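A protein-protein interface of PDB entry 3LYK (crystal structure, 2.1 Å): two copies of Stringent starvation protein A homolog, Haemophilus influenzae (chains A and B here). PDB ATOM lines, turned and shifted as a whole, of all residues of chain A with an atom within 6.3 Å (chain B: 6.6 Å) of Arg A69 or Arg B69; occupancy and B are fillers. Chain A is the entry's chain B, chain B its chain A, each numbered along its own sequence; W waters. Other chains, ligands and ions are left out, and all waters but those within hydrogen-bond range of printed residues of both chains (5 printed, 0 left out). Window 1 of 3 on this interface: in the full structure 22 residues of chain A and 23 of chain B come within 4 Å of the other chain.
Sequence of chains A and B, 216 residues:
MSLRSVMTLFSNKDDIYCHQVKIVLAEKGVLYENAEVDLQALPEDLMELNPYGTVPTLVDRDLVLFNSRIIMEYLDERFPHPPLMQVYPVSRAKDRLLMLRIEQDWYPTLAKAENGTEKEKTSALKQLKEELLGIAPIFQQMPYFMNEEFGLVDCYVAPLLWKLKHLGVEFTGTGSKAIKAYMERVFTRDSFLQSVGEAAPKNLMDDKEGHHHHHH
Asn A67 touches Leu B100, and with the chains exchanged Leu A100 touches Asn B67. Arg A69 touches its own counterpart, Arg B69. Ile A70 touches Arg B96, and with the chains exchanged Arg A96 touches Ile B70. Glu A73 touches Arg B96, and with the chains exchanged Arg A96 touches Glu B73. Positions printed for both chains: 20, 21, 66, 67, 68, 69, 70, 71, 72, 73, 74, 96, 100, 152 and 156. Of the 8 pairs that touch across the chains among the printed residues, 7 have their exchanged pair printed and touching as well.
Water W3 lies within hydrogen-bond range of NH1 of Arg B96 (2.7 Å), O of Ile A70 (2.9 Å) and N of Tyr A74 (3.3 Å). Water W1 lies within hydrogen-bond range of the side-chain carboxylate of Glu A73, the side-chain carboxylate of Glu B73 and the guanidinium group of Arg A69. Water W5 bridges the backbone carbonyl oxygen (O) of Arg A96 (3.0 Å) and the guanidinium group (NH1) of Arg B69 (3.4 Å). Water W4 lies within hydrogen-bond range of O of Ile B70, NH1 of Arg A96 and N of Tyr B74. Water W2 bridges O of Arg B96 (3.2 Å) and NH1 of Arg A69 (3.5 Å).
NH2 of Arg A96 lies within salt-bridge range of OE1 of Glu B73, at 3.7 Å. NH2 of Arg B96 is in salt-bridge range of OE1 of Glu A73.
Among the printed residues, pairs that only touch across the chains: Asn A67 with Leu B100, Arg A69 with Arg B69, Ile A70 with Arg B96, Arg A96 with Ile B70, Leu A100 with Asn B67 and Leu A100 with Ile B70.
Of the printed residues of chain B, Asn A67 touches Leu B100. Of chain B, only Arg B69 comes within 4 Å of Arg A69. Met A72 touches none of the printed residues of chain B. Printed residues of chain B within 4 Å of Arg A96: Ile B70 and Glu B73. Of the printed residues of chain B, Leu A100 touches Asn B67 (3.7 Å) and Ile B70 (3.9 Å). Of chain A, only Arg A69 comes within 4 Å of Arg B69. Of the printed residues of chain A, Ile B70 touches Arg A96 (3.6 Å) and Leu A100 (3.9 Å). The nearest residue of chain A that does not touch Arg B69 is Leu A100 (4.2 Å). The nearest printed residue of chain A that does not touch Glu B73 is Glu A73 (4.7 Å).
Hydrophobic or aromatic side chains of chain A within 4 Å of the printed part of chain B: Ile A70 and Leu A100. Printed residues of chain B that touch a printed residue of chain A: Asn B67, Arg B69, Ile B70, Glu B73, Arg B96 and Leu B100. Hydrophobic or aromatic side chains of chain B within 4 Å of the printed part of chain A: Ile B70 and Leu B100.
The side-chain amide oxygen of Asn B67 lies within hydrogen-bond range of the backbone NH of Arg B69, at 3.2 Å. The side-chain amide oxygen of Asn B67 is in hydrogen-bond range of the backbone NH of Ile B70 (3.2 Å). OE2 of Glu B73 lies within salt-bridge range of NE of Arg B96 (2.8 Å). OD1 of Asn A67 lies within hydrogen-bond range of N of Arg A69. OD1 of Asn A67 is in hydrogen-bond range of N of Ile A70 (3.0 Å). NH2 of Arg A96 lies within salt-bridge range of OE1 of Glu A73, 2.7 Å away.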
ATOM      1  N   GLN A  20     -32.918  18.585  24.847  1.00  0.00           N
ATOM      2  CA  GLN A  20     -31.803  17.926  24.165  1.00  0.00           C
ATOM      3  C   GLN A  20     -30.519  17.923  25.031  1.00  0.00           C
ATOM      4  O   GLN A  20     -29.849  16.889  25.174  1.00  0.00           O
ATOM      5  CB  GLN A  20     -31.449  18.649  22.843  1.00  0.00           C
ATOM      6  CG  GLN A  20     -32.550  18.716  21.799  1.00  0.00           C
ATOM      7  CD  GLN A  20     -32.103  19.563  20.595  1.00  0.00           C
ATOM      8  OE1 GLN A  20     -31.250  20.441  20.719  1.00  0.00           O
ATOM      9  NE2 GLN A  20     -32.702  19.326  19.466  1.00  0.00           N
ATOM     10  N   VAL A  21     -30.168  19.101  25.545  1.00  0.00           N
ATOM     11  CA  VAL A  21     -28.956  19.271  26.305  1.00  0.00           C
ATOM     12  C   VAL A  21     -28.996  18.465  27.630  1.00  0.00           C
ATOM     13  O   VAL A  21     -28.000  17.781  28.000  1.00  0.00           O
ATOM     14  CB  VAL A  21     -28.653  20.785  26.575  1.00  0.00           C
ATOM     15  CG1 VAL A  21     -27.443  20.950  27.526  1.00  0.00           C
ATOM     16  CG2 VAL A  21     -28.310  21.504  25.236  1.00  0.00           C
ATOM     17  N   PHE A  66     -23.806  28.881  24.369  1.00  0.00           N
ATOM     18  CA  PHE A  66     -25.235  28.787  24.071  1.00  0.00           C
ATOM     19  C   PHE A  66     -25.321  28.169  22.707  1.00  0.00           C
ATOM     20  O   PHE A  66     -24.268  27.930  22.065  1.00  0.00           O
ATOM     21  CB  PHE A  66     -25.938  30.148  24.128  1.00  0.00           C
ATOM     22  CG  PHE A  66     -25.207  31.238  23.395  1.00  0.00           C
ATOM     23  CD1 PHE A  66     -25.484  31.495  22.054  1.00  0.00           C
ATOM     24  CD2 PHE A  66     -24.206  31.968  24.037  1.00  0.00           C
ATOM     25  CE1 PHE A  66     -24.796  32.498  21.362  1.00  0.00           C
ATOM     26  CE2 PHE A  66     -23.510  32.983  23.351  1.00  0.00           C
ATOM     27  CZ  PHE A  66     -23.808  33.232  22.017  1.00  0.00           C
ATOM     28  N   ASN A  67     -26.543  27.933  22.246  1.00  0.00           N
ATOM     29  CA  ASN A  67     -26.832  27.034  21.124  1.00  0.00           C
ATOM     30  C   ASN A  67     -26.639  25.573  21.498  1.00  0.00           C
ATOM     31  O   ASN A  67     -25.528  25.126  21.833  1.00  0.00           O
ATOM     32  CB  ASN A  67     -26.021  27.388  19.849  1.00  0.00           C
ATOM     33  CG  ASN A  67     -26.389  26.521  18.680  1.00  0.00           C
ATOM     34  OD1 ASN A  67     -25.952  25.375  18.590  1.00  0.00           O
ATOM     35  ND2 ASN A  67     -27.211  27.049  17.771  1.00  0.00           N
ATOM     36  N   SER A  68     -27.723  24.808  21.391  1.00  0.00           N
ATOM     37  CA  SER A  68     -27.718  23.460  21.927  1.00  0.00           C
ATOM     38  C   SER A  68     -26.811  22.547  21.102  1.00  0.00           C
ATOM     39  O   SER A  68     -26.159  21.681  21.659  1.00  0.00           O
ATOM     40  CB  SER A  68     -29.130  22.905  22.056  1.00  0.00           C
ATOM     41  OG  SER A  68     -29.681  22.720  20.785  1.00  0.00           O
ATOM     42  N   ARG A  69     -26.739  22.755  19.781  1.00  0.00           N
ATOM     43  CA  ARG A  69     -25.827  21.914  18.954  1.00  0.00           C
ATOM     44  C   ARG A  69     -24.356  22.123  19.383  1.00  0.00           C
ATOM     45  O   ARG A  69     -23.609  21.182  19.547  1.00  0.00           O
ATOM     46  CB  ARG A  69     -26.050  22.179  17.443  1.00  0.00           C
ATOM     47  CG  ARG A  69     -24.913  21.738  16.537  1.00  0.00           C
ATOM     48  CD  ARG A  69     -25.088  22.330  15.083  1.00  0.00           C
ATOM     49  NE  ARG A  69     -25.090  23.803  15.054  1.00  0.00           N
ATOM     50  CZ  ARG A  69     -24.002  24.579  14.989  1.00  0.00           C
ATOM     51  NH1 ARG A  69     -22.795  24.047  14.976  1.00  0.00           N
ATOM     52  NH2 ARG A  69     -24.115  25.898  14.948  1.00  0.00           N
ATOM     53  N   ILE A  70     -23.962  23.351  19.612  1.00  0.00           N
ATOM     54  CA  ILE A  70     -22.604  23.630  20.042  1.00  0.00           C
ATOM     55  C   ILE A  70     -22.347  23.047  21.424  1.00  0.00           C
ATOM     56  O   ILE A  70     -21.276  22.482  21.699  1.00  0.00           O
ATOM     57  CB  ILE A  70     -22.329  25.137  20.059  1.00  0.00           C
ATOM     58  CG1 ILE A  70     -22.354  25.663  18.612  1.00  0.00           C
ATOM     59  CG2 ILE A  70     -20.958  25.447  20.710  1.00  0.00           C
ATOM     60  CD1 ILE A  70     -21.982  27.113  18.506  1.00  0.00           C
ATOM     61  N   ILE A  71     -23.317  23.221  22.319  1.00  0.00           N
ATOM     62  CA  ILE A  71     -23.213  22.599  23.651  1.00  0.00           C
ATOM     63  C   ILE A  71     -23.064  21.076  23.608  1.00  0.00           C
ATOM     64  O   ILE A  71     -22.195  20.500  24.278  1.00  0.00           O
ATOM     65  CB  ILE A  71     -24.412  23.032  24.547  1.00  0.00           C
ATOM     66  CG1 ILE A  71     -24.197  24.495  24.963  1.00  0.00           C
ATOM     67  CG2 ILE A  71     -24.553  22.091  25.807  1.00  0.00           C
ATOM     68  CD1 ILE A  71     -25.478  25.145  25.545  1.00  0.00           C
ATOM     69  N   MET A  72     -23.905  20.427  22.832  1.00  0.00           N
ATOM     70  CA  MET A  72     -23.893  18.968  22.765  1.00  0.00           C
ATOM     71  C   MET A  72     -22.620  18.409  22.196  1.00  0.00           C
ATOM     72  O   MET A  72     -22.094  17.394  22.696  1.00  0.00           O
ATOM     73  CB  MET A  72     -25.111  18.438  21.978  1.00  0.00           C
ATOM     74  CG  MET A  72     -26.443  18.677  22.772  1.00  0.00           C
ATOM     75  SD  MET A  72     -27.913  17.846  21.759  1.00  0.00           S
ATOM     76  CE  MET A  72     -28.133  19.321  20.593  1.00  0.00           C
ATOM     77  N   GLU A  73     -22.119  19.053  21.140  1.00  0.00           N
ATOM     78  CA  GLU A  73     -20.840  18.609  20.593  1.00  0.00           C
ATOM     79  C   GLU A  73     -19.708  18.883  21.551  1.00  0.00           C
ATOM     80  O   GLU A  73     -18.840  18.058  21.692  1.00  0.00           O
ATOM     81  CB  GLU A  73     -20.579  19.194  19.189  1.00  0.00           C
ATOM     82  CG  GLU A  73     -21.466  18.461  18.118  1.00  0.00           C
ATOM     83  CD  GLU A  73     -20.810  18.391  16.700  1.00  0.00           C
ATOM     84  OE1 GLU A  73     -19.594  18.012  16.608  1.00  0.00           O
ATOM     85  OE2 GLU A  73     -21.535  18.700  15.702  1.00  0.00           O
ATOM     86  N   TYR A  74     -19.718  20.029  22.223  1.00  0.00           N
ATOM     87  CA  TYR A  74     -18.759  20.256  23.297  1.00  0.00           C
ATOM     88  C   TYR A  74     -18.754  19.134  24.356  1.00  0.00           C
ATOM     89  O   TYR A  74     -17.681  18.644  24.792  1.00  0.00           O
ATOM     90  CB  TYR A  74     -19.053  21.614  23.946  1.00  0.00           C
ATOM     91  CG  TYR A  74     -18.331  21.832  25.284  1.00  0.00           C
ATOM     92  CD1 TYR A  74     -16.945  22.057  25.324  1.00  0.00           C
ATOM     93  CD2 TYR A  74     -19.033  21.791  26.506  1.00  0.00           C
ATOM     94  CE1 TYR A  74     -16.256  22.239  26.558  1.00  0.00           C
ATOM     95  CE2 TYR A  74     -18.367  21.967  27.711  1.00  0.00           C
ATOM     96  CZ  TYR A  74     -16.984  22.196  27.730  1.00  0.00           C
ATOM     97  OH  TYR A  74     -16.330  22.394  28.918  1.00  0.00           O
ATOM     98  N   ARG A  96     -25.011  14.655  11.311  1.00  0.00           N
ATOM     99  CA  ARG A  96     -25.168  16.103  11.365  1.00  0.00           C
ATOM    100  C   ARG A  96     -26.250  16.594  10.416  1.00  0.00           C
ATOM    101  O   ARG A  96     -27.028  17.519  10.742  1.00  0.00           O
ATOM    102  CB  ARG A  96     -23.834  16.821  11.072  1.00  0.00           C
ATOM    103  CG  ARG A  96     -22.840  16.807  12.270  1.00  0.00           C
ATOM    104  CD  ARG A  96     -21.731  17.798  12.065  1.00  0.00           C
ATOM    105  NE  ARG A  96     -20.776  17.727  13.165  1.00  0.00           N
ATOM    106  CZ  ARG A  96     -19.562  17.180  13.073  1.00  0.00           C
ATOM    107  NH1 ARG A  96     -19.137  16.652  11.911  1.00  0.00           N
ATOM    108  NH2 ARG A  96     -18.754  17.185  14.136  1.00  0.00           N
ATOM    109  N   LEU A 100     -29.827  18.504  11.303  1.00  0.00           N
ATOM    110  CA  LEU A 100     -30.211  19.757  10.703  1.00  0.00           C
ATOM    111  C   LEU A 100     -31.605  19.644  10.094  1.00  0.00           C
ATOM    112  O   LEU A 100     -32.422  20.562  10.248  1.00  0.00           O
ATOM    113  CB  LEU A 100     -29.239  20.162   9.598  1.00  0.00           C
ATOM    114  CG  LEU A 100     -29.705  21.365   8.763  1.00  0.00           C
ATOM    115  CD1 LEU A 100     -29.649  22.613   9.603  1.00  0.00           C
ATOM    116  CD2 LEU A 100     -28.804  21.573   7.496  1.00  0.00           C
ATOM    117  N   LEU A 152     -26.604  11.401  19.337  1.00  0.00           N
ATOM    118  CA  LEU A 152     -27.140  12.763  19.248  1.00  0.00           C
ATOM    119  C   LEU A 152     -28.379  12.896  18.376  1.00  0.00           C
ATOM    120  O   LEU A 152     -29.218  13.738  18.665  1.00  0.00           O
ATOM    121  CB  LEU A 152     -26.062  13.780  18.828  1.00  0.00           C
ATOM    122  CG  LEU A 152     -24.856  13.978  19.760  1.00  0.00           C
ATOM    123  CD1 LEU A 152     -23.910  15.130  19.229  1.00  0.00           C
ATOM    124  CD2 LEU A 152     -25.286  14.262  21.216  1.00  0.00           C
ATOM    125  N   TYR A 156     -32.305  14.485  19.259  1.00  0.00           N
ATOM    126  CA  TYR A 156     -33.207  15.390  18.540  1.00  0.00           C
ATOM    127  C   TYR A 156     -34.603  14.755  18.402  1.00  0.00           C
ATOM    128  O   TYR A 156     -35.599  15.444  18.506  1.00  0.00           O
ATOM    129  CB  TYR A 156     -32.681  15.741  17.111  1.00  0.00           C
ATOM    130  CG  TYR A 156     -31.672  16.880  17.065  1.00  0.00           C
ATOM    131  CD1 TYR A 156     -30.390  16.713  17.601  1.00  0.00           C
ATOM    132  CD2 TYR A 156     -31.991  18.112  16.482  1.00  0.00           C
ATOM    133  CE1 TYR A 156     -29.458  17.735  17.584  1.00  0.00           C
ATOM    134  CE2 TYR A 156     -31.031  19.172  16.455  1.00  0.00           C
ATOM    135  CZ  TYR A 156     -29.779  18.958  17.007  1.00  0.00           C
ATOM    136  OH  TYR A 156     -28.815  19.936  17.018  1.00  0.00           O
ATOM    137  N   GLN B  20     -16.859  30.137   1.463  1.00  0.00           N
ATOM    138  CA  GLN B  20     -16.310  29.440   2.648  1.00  0.00           C
ATOM    139  C   GLN B  20     -15.825  28.041   2.307  1.00  0.00           C
ATOM    140  O   GLN B  20     -14.743  27.640   2.709  1.00  0.00           O
ATOM    141  CB  GLN B  20     -17.387  29.263   3.739  1.00  0.00           C
ATOM    142  CG  GLN B  20     -17.979  30.556   4.299  1.00  0.00           C
ATOM    143  CD  GLN B  20     -19.180  30.304   5.241  1.00  0.00           C
ATOM    144  OE1 GLN B  20     -19.902  29.331   5.103  1.00  0.00           O
ATOM    145  NE2 GLN B  20     -19.401  31.215   6.156  1.00  0.00           N
ATOM    146  N   VAL B  21     -16.657  27.276   1.622  1.00  0.00           N
ATOM    147  CA  VAL B  21     -16.369  25.878   1.381  1.00  0.00           C
ATOM    148  C   VAL B  21     -15.166  25.788   0.402  1.00  0.00           C
ATOM    149  O   VAL B  21     -14.231  25.014   0.588  1.00  0.00           O
ATOM    150  CB  VAL B  21     -17.625  25.206   0.773  1.00  0.00           C
ATOM    151  CG1 VAL B  21     -17.329  23.838   0.235  1.00  0.00           C
ATOM    152  CG2 VAL B  21     -18.788  25.155   1.793  1.00  0.00           C
ATOM    153  N   PHE B  66     -25.171  19.364   2.346  1.00  0.00           N
ATOM    154  CA  PHE B  66     -25.445  20.759   2.146  1.00  0.00           C
ATOM    155  C   PHE B  66     -25.342  21.453   3.460  1.00  0.00           C
ATOM    156  O   PHE B  66     -25.205  20.777   4.501  1.00  0.00           O
ATOM    157  CB  PHE B  66     -26.797  21.008   1.468  1.00  0.00           C
ATOM    158  CG  PHE B  66     -27.903  20.142   1.987  1.00  0.00           C
ATOM    159  CD1 PHE B  66     -28.670  20.556   3.081  1.00  0.00           C
ATOM    160  CD2 PHE B  66     -28.163  18.913   1.400  1.00  0.00           C
ATOM    161  CE1 PHE B  66     -29.690  19.774   3.556  1.00  0.00           C
ATOM    162  CE2 PHE B  66     -29.185  18.111   1.870  1.00  0.00           C
ATOM    163  CZ  PHE B  66     -29.946  18.542   2.955  1.00  0.00           C
ATOM    164  N   ASN B  67     -25.436  22.776   3.421  1.00  0.00           N
ATOM    165  CA  ASN B  67     -25.178  23.642   4.555  1.00  0.00           C
ATOM    166  C   ASN B  67     -23.667  23.775   4.763  1.00  0.00           C
ATOM    167  O   ASN B  67     -22.966  22.771   4.948  1.00  0.00           O
ATOM    168  CB  ASN B  67     -25.912  23.145   5.819  1.00  0.00           C
ATOM    169  CG  ASN B  67     -25.587  23.962   7.013  1.00  0.00           C
ATOM    170  OD1 ASN B  67     -24.509  23.804   7.596  1.00  0.00           O
ATOM    171  ND2 ASN B  67     -26.505  24.833   7.418  1.00  0.00           N
ATOM    172  N   SER B  68     -23.140  25.002   4.659  1.00  0.00           N
ATOM    173  CA  SER B  68     -21.712  25.136   4.540  1.00  0.00           C
ATOM    174  C   SER B  68     -20.975  24.681   5.824  1.00  0.00           C
ATOM    175  O   SER B  68     -19.873  24.147   5.749  1.00  0.00           O
ATOM    176  CB  SER B  68     -21.326  26.545   4.119  1.00  0.00           C
ATOM    177  OG  SER B  68     -21.749  27.468   5.082  1.00  0.00           O
ATOM    178  N   ARG B  69     -21.605  24.903   6.988  1.00  0.00           N
ATOM    179  CA  ARG B  69     -21.021  24.475   8.270  1.00  0.00           C
ATOM    180  C   ARG B  69     -20.792  22.956   8.330  1.00  0.00           C
ATOM    181  O   ARG B  69     -19.726  22.488   8.768  1.00  0.00           O
ATOM    182  CB  ARG B  69     -21.891  24.974   9.433  1.00  0.00           C
ATOM    183  CG  ARG B  69     -21.615  24.298  10.767  1.00  0.00           C
ATOM    184  CD  ARG B  69     -22.672  24.767  11.833  1.00  0.00           C
ATOM    185  NE  ARG B  69     -24.082  24.395  11.582  1.00  0.00           N
ATOM    186  CZ  ARG B  69     -24.606  23.167  11.741  1.00  0.00           C
ATOM    187  NH1 ARG B  69     -23.870  22.103  12.088  1.00  0.00           N
ATOM    188  NH2 ARG B  69     -25.885  22.990  11.512  1.00  0.00           N
ATOM    189  N   ILE B  70     -21.755  22.191   7.844  1.00  0.00           N
ATOM    190  CA  ILE B  70     -21.667  20.729   7.866  1.00  0.00           C
ATOM    191  C   ILE B  70     -20.597  20.237   6.863  1.00  0.00           C
ATOM    192  O   ILE B  70     -19.797  19.341   7.164  1.00  0.00           O
ATOM    193  CB  ILE B  70     -23.053  20.116   7.580  1.00  0.00           C
ATOM    194  CG1 ILE B  70     -23.941  20.334   8.834  1.00  0.00           C
ATOM    195  CG2 ILE B  70     -22.954  18.648   7.290  1.00  0.00           C
ATOM    196  CD1 ILE B  70     -25.410  19.950   8.656  1.00  0.00           C
ATOM    197  N   ILE B  71     -20.568  20.874   5.689  1.00  0.00           N
ATOM    198  CA  ILE B  71     -19.554  20.570   4.670  1.00  0.00           C
ATOM    199  C   ILE B  71     -18.145  20.828   5.183  1.00  0.00           C
ATOM    200  O   ILE B  71     -17.288  19.983   5.062  1.00  0.00           O
ATOM    201  CB  ILE B  71     -19.824  21.412   3.397  1.00  0.00           C
ATOM    202  CG1 ILE B  71     -21.119  20.900   2.744  1.00  0.00           C
ATOM    203  CG2 ILE B  71     -18.623  21.320   2.406  1.00  0.00           C
ATOM    204  CD1 ILE B  71     -21.681  21.797   1.641  1.00  0.00           C
ATOM    205  N   MET B  72     -17.923  22.002   5.756  1.00  0.00           N
ATOM    206  CA  MET B  72     -16.632  22.345   6.321  1.00  0.00           C
ATOM    207  C   MET B  72     -16.155  21.414   7.416  1.00  0.00           C
ATOM    208  O   MET B  72     -14.988  21.040   7.445  1.00  0.00           O
ATOM    209  CB  MET B  72     -16.628  23.811   6.814  1.00  0.00           C
ATOM    210  CG  MET B  72     -16.707  24.815   5.615  1.00  0.00           C
ATOM    211  SD  MET B  72     -16.414  26.637   6.266  1.00  0.00           S
ATOM    212  CE  MET B  72     -18.198  27.026   6.830  1.00  0.00           C
ATOM    213  N   GLU B  73     -17.065  21.011   8.301  1.00  0.00           N
ATOM    214  CA  GLU B  73     -16.687  20.112   9.373  1.00  0.00           C
ATOM    215  C   GLU B  73     -16.387  18.741   8.807  1.00  0.00           C
ATOM    216  O   GLU B  73     -15.402  18.132   9.187  1.00  0.00           O
ATOM    217  CB  GLU B  73     -17.760  20.118  10.492  1.00  0.00           C
ATOM    218  CG  GLU B  73     -17.698  21.467  11.292  1.00  0.00           C
ATOM    219  CD  GLU B  73     -17.710  21.309  12.835  1.00  0.00           C
ATOM    220  OE1 GLU B  73     -17.086  20.348  13.354  1.00  0.00           O
ATOM    221  OE2 GLU B  73     -18.308  22.177  13.531  1.00  0.00           O
ATOM    222  N   TYR B  74     -17.203  18.291   7.847  1.00  0.00           N
ATOM    223  CA  TYR B  74     -16.915  17.061   7.144  1.00  0.00           C
ATOM    224  C   TYR B  74     -15.493  17.094   6.480  1.00  0.00           C
ATOM    225  O   TYR B  74     -14.685  16.196   6.650  1.00  0.00           O
ATOM    226  CB  TYR B  74     -17.978  16.823   6.058  1.00  0.00           C
ATOM    227  CG  TYR B  74     -17.550  15.670   5.167  1.00  0.00           C
ATOM    228  CD1 TYR B  74     -17.472  14.368   5.679  1.00  0.00           C
ATOM    229  CD2 TYR B  74     -17.152  15.880   3.839  1.00  0.00           C
ATOM    230  CE1 TYR B  74     -17.052  13.300   4.885  1.00  0.00           C
ATOM    231  CE2 TYR B  74     -16.701  14.784   3.010  1.00  0.00           C
ATOM    232  CZ  TYR B  74     -16.646  13.526   3.548  1.00  0.00           C
ATOM    233  OH  TYR B  74     -16.243  12.442   2.782  1.00  0.00           O
ATOM    234  N   ARG B  96     -16.494  27.525  17.381  1.00  0.00           N
ATOM    235  CA  ARG B  96     -17.856  27.334  16.892  1.00  0.00           C
ATOM    236  C   ARG B  96     -18.784  28.467  17.248  1.00  0.00           C
ATOM    237  O   ARG B  96     -19.604  28.888  16.409  1.00  0.00           O
ATOM    238  CB  ARG B  96     -18.452  26.017  17.303  1.00  0.00           C
ATOM    239  CG  ARG B  96     -17.772  24.825  16.629  1.00  0.00           C
ATOM    240  CD  ARG B  96     -18.543  23.607  16.969  1.00  0.00           C
ATOM    241  NE  ARG B  96     -18.057  22.414  16.296  1.00  0.00           N
ATOM    242  CZ  ARG B  96     -17.559  21.340  16.923  1.00  0.00           C
ATOM    243  NH1 ARG B  96     -17.456  21.313  18.260  1.00  0.00           N
ATOM    244  NH2 ARG B  96     -17.157  20.294  16.208  1.00  0.00           N
ATOM    245  N   LEU B 100     -20.762  31.028  14.733  1.00  0.00           N
ATOM    246  CA  LEU B 100     -22.209  31.223  14.846  1.00  0.00           C
ATOM    247  C   LEU B 100     -22.546  32.726  14.943  1.00  0.00           C
ATOM    248  O   LEU B 100     -23.446  33.205  14.262  1.00  0.00           O
ATOM    249  CB  LEU B 100     -22.782  30.447  16.059  1.00  0.00           C
ATOM    250  CG  LEU B 100     -24.287  30.661  16.297  1.00  0.00           C
ATOM    251  CD1 LEU B 100     -25.098  29.953  15.210  1.00  0.00           C
ATOM    252  CD2 LEU B 100     -24.725  30.137  17.686  1.00  0.00           C
ATOM    253  N   LEU B 152     -10.972  27.534  10.565  1.00  0.00           N
ATOM    254  CA  LEU B 152     -12.350  27.736  10.100  1.00  0.00           C
ATOM    255  C   LEU B 152     -12.932  29.091  10.445  1.00  0.00           C
ATOM    256  O   LEU B 152     -13.756  29.634   9.689  1.00  0.00           O
ATOM    257  CB  LEU B 152     -13.326  26.609  10.557  1.00  0.00           C
ATOM    258  CG  LEU B 152     -13.045  25.198   9.984  1.00  0.00           C
ATOM    259  CD1 LEU B 152     -14.139  24.136  10.482  1.00  0.00           C
ATOM    260  CD2 LEU B 152     -12.987  25.232   8.479  1.00  0.00           C
ATOM    261  N   TYR B 156     -14.874  32.243   7.914  1.00  0.00           N
ATOM    262  CA  TYR B 156     -16.108  33.059   8.046  1.00  0.00           C
ATOM    263  C   TYR B 156     -15.756  34.521   7.878  1.00  0.00           C
ATOM    264  O   TYR B 156     -16.499  35.268   7.265  1.00  0.00           O
ATOM    265  CB  TYR B 156     -16.773  32.898   9.460  1.00  0.00           C
ATOM    266  CG  TYR B 156     -17.635  31.685   9.544  1.00  0.00           C
ATOM    267  CD1 TYR B 156     -17.060  30.425   9.517  1.00  0.00           C
ATOM    268  CD2 TYR B 156     -19.037  31.787   9.562  1.00  0.00           C
ATOM    269  CE1 TYR B 156     -17.852  29.276   9.552  1.00  0.00           C
ATOM    270  CE2 TYR B 156     -19.861  30.626   9.595  1.00  0.00           C
ATOM    271  CZ  TYR B 156     -19.237  29.384   9.606  1.00  0.00           C
ATOM    272  OH  TYR B 156     -19.949  28.220   9.624  1.00  0.00           O
HETATM  273  O   HOH W   1     -21.086  21.324  14.391  1.00  0.00           O
HETATM  274  O   HOH W   2     -20.663  26.707  14.331  1.00  0.00           O
HETATM  275  O   HOH W   3     -18.635  22.579  20.395  1.00  0.00           O
HETATM  276  O   HOH W   4     -19.896  17.016   9.039  1.00  0.00           O
HETATM  277  O   HOH W   5     -26.090  19.561  12.681  1.00  0.00           O
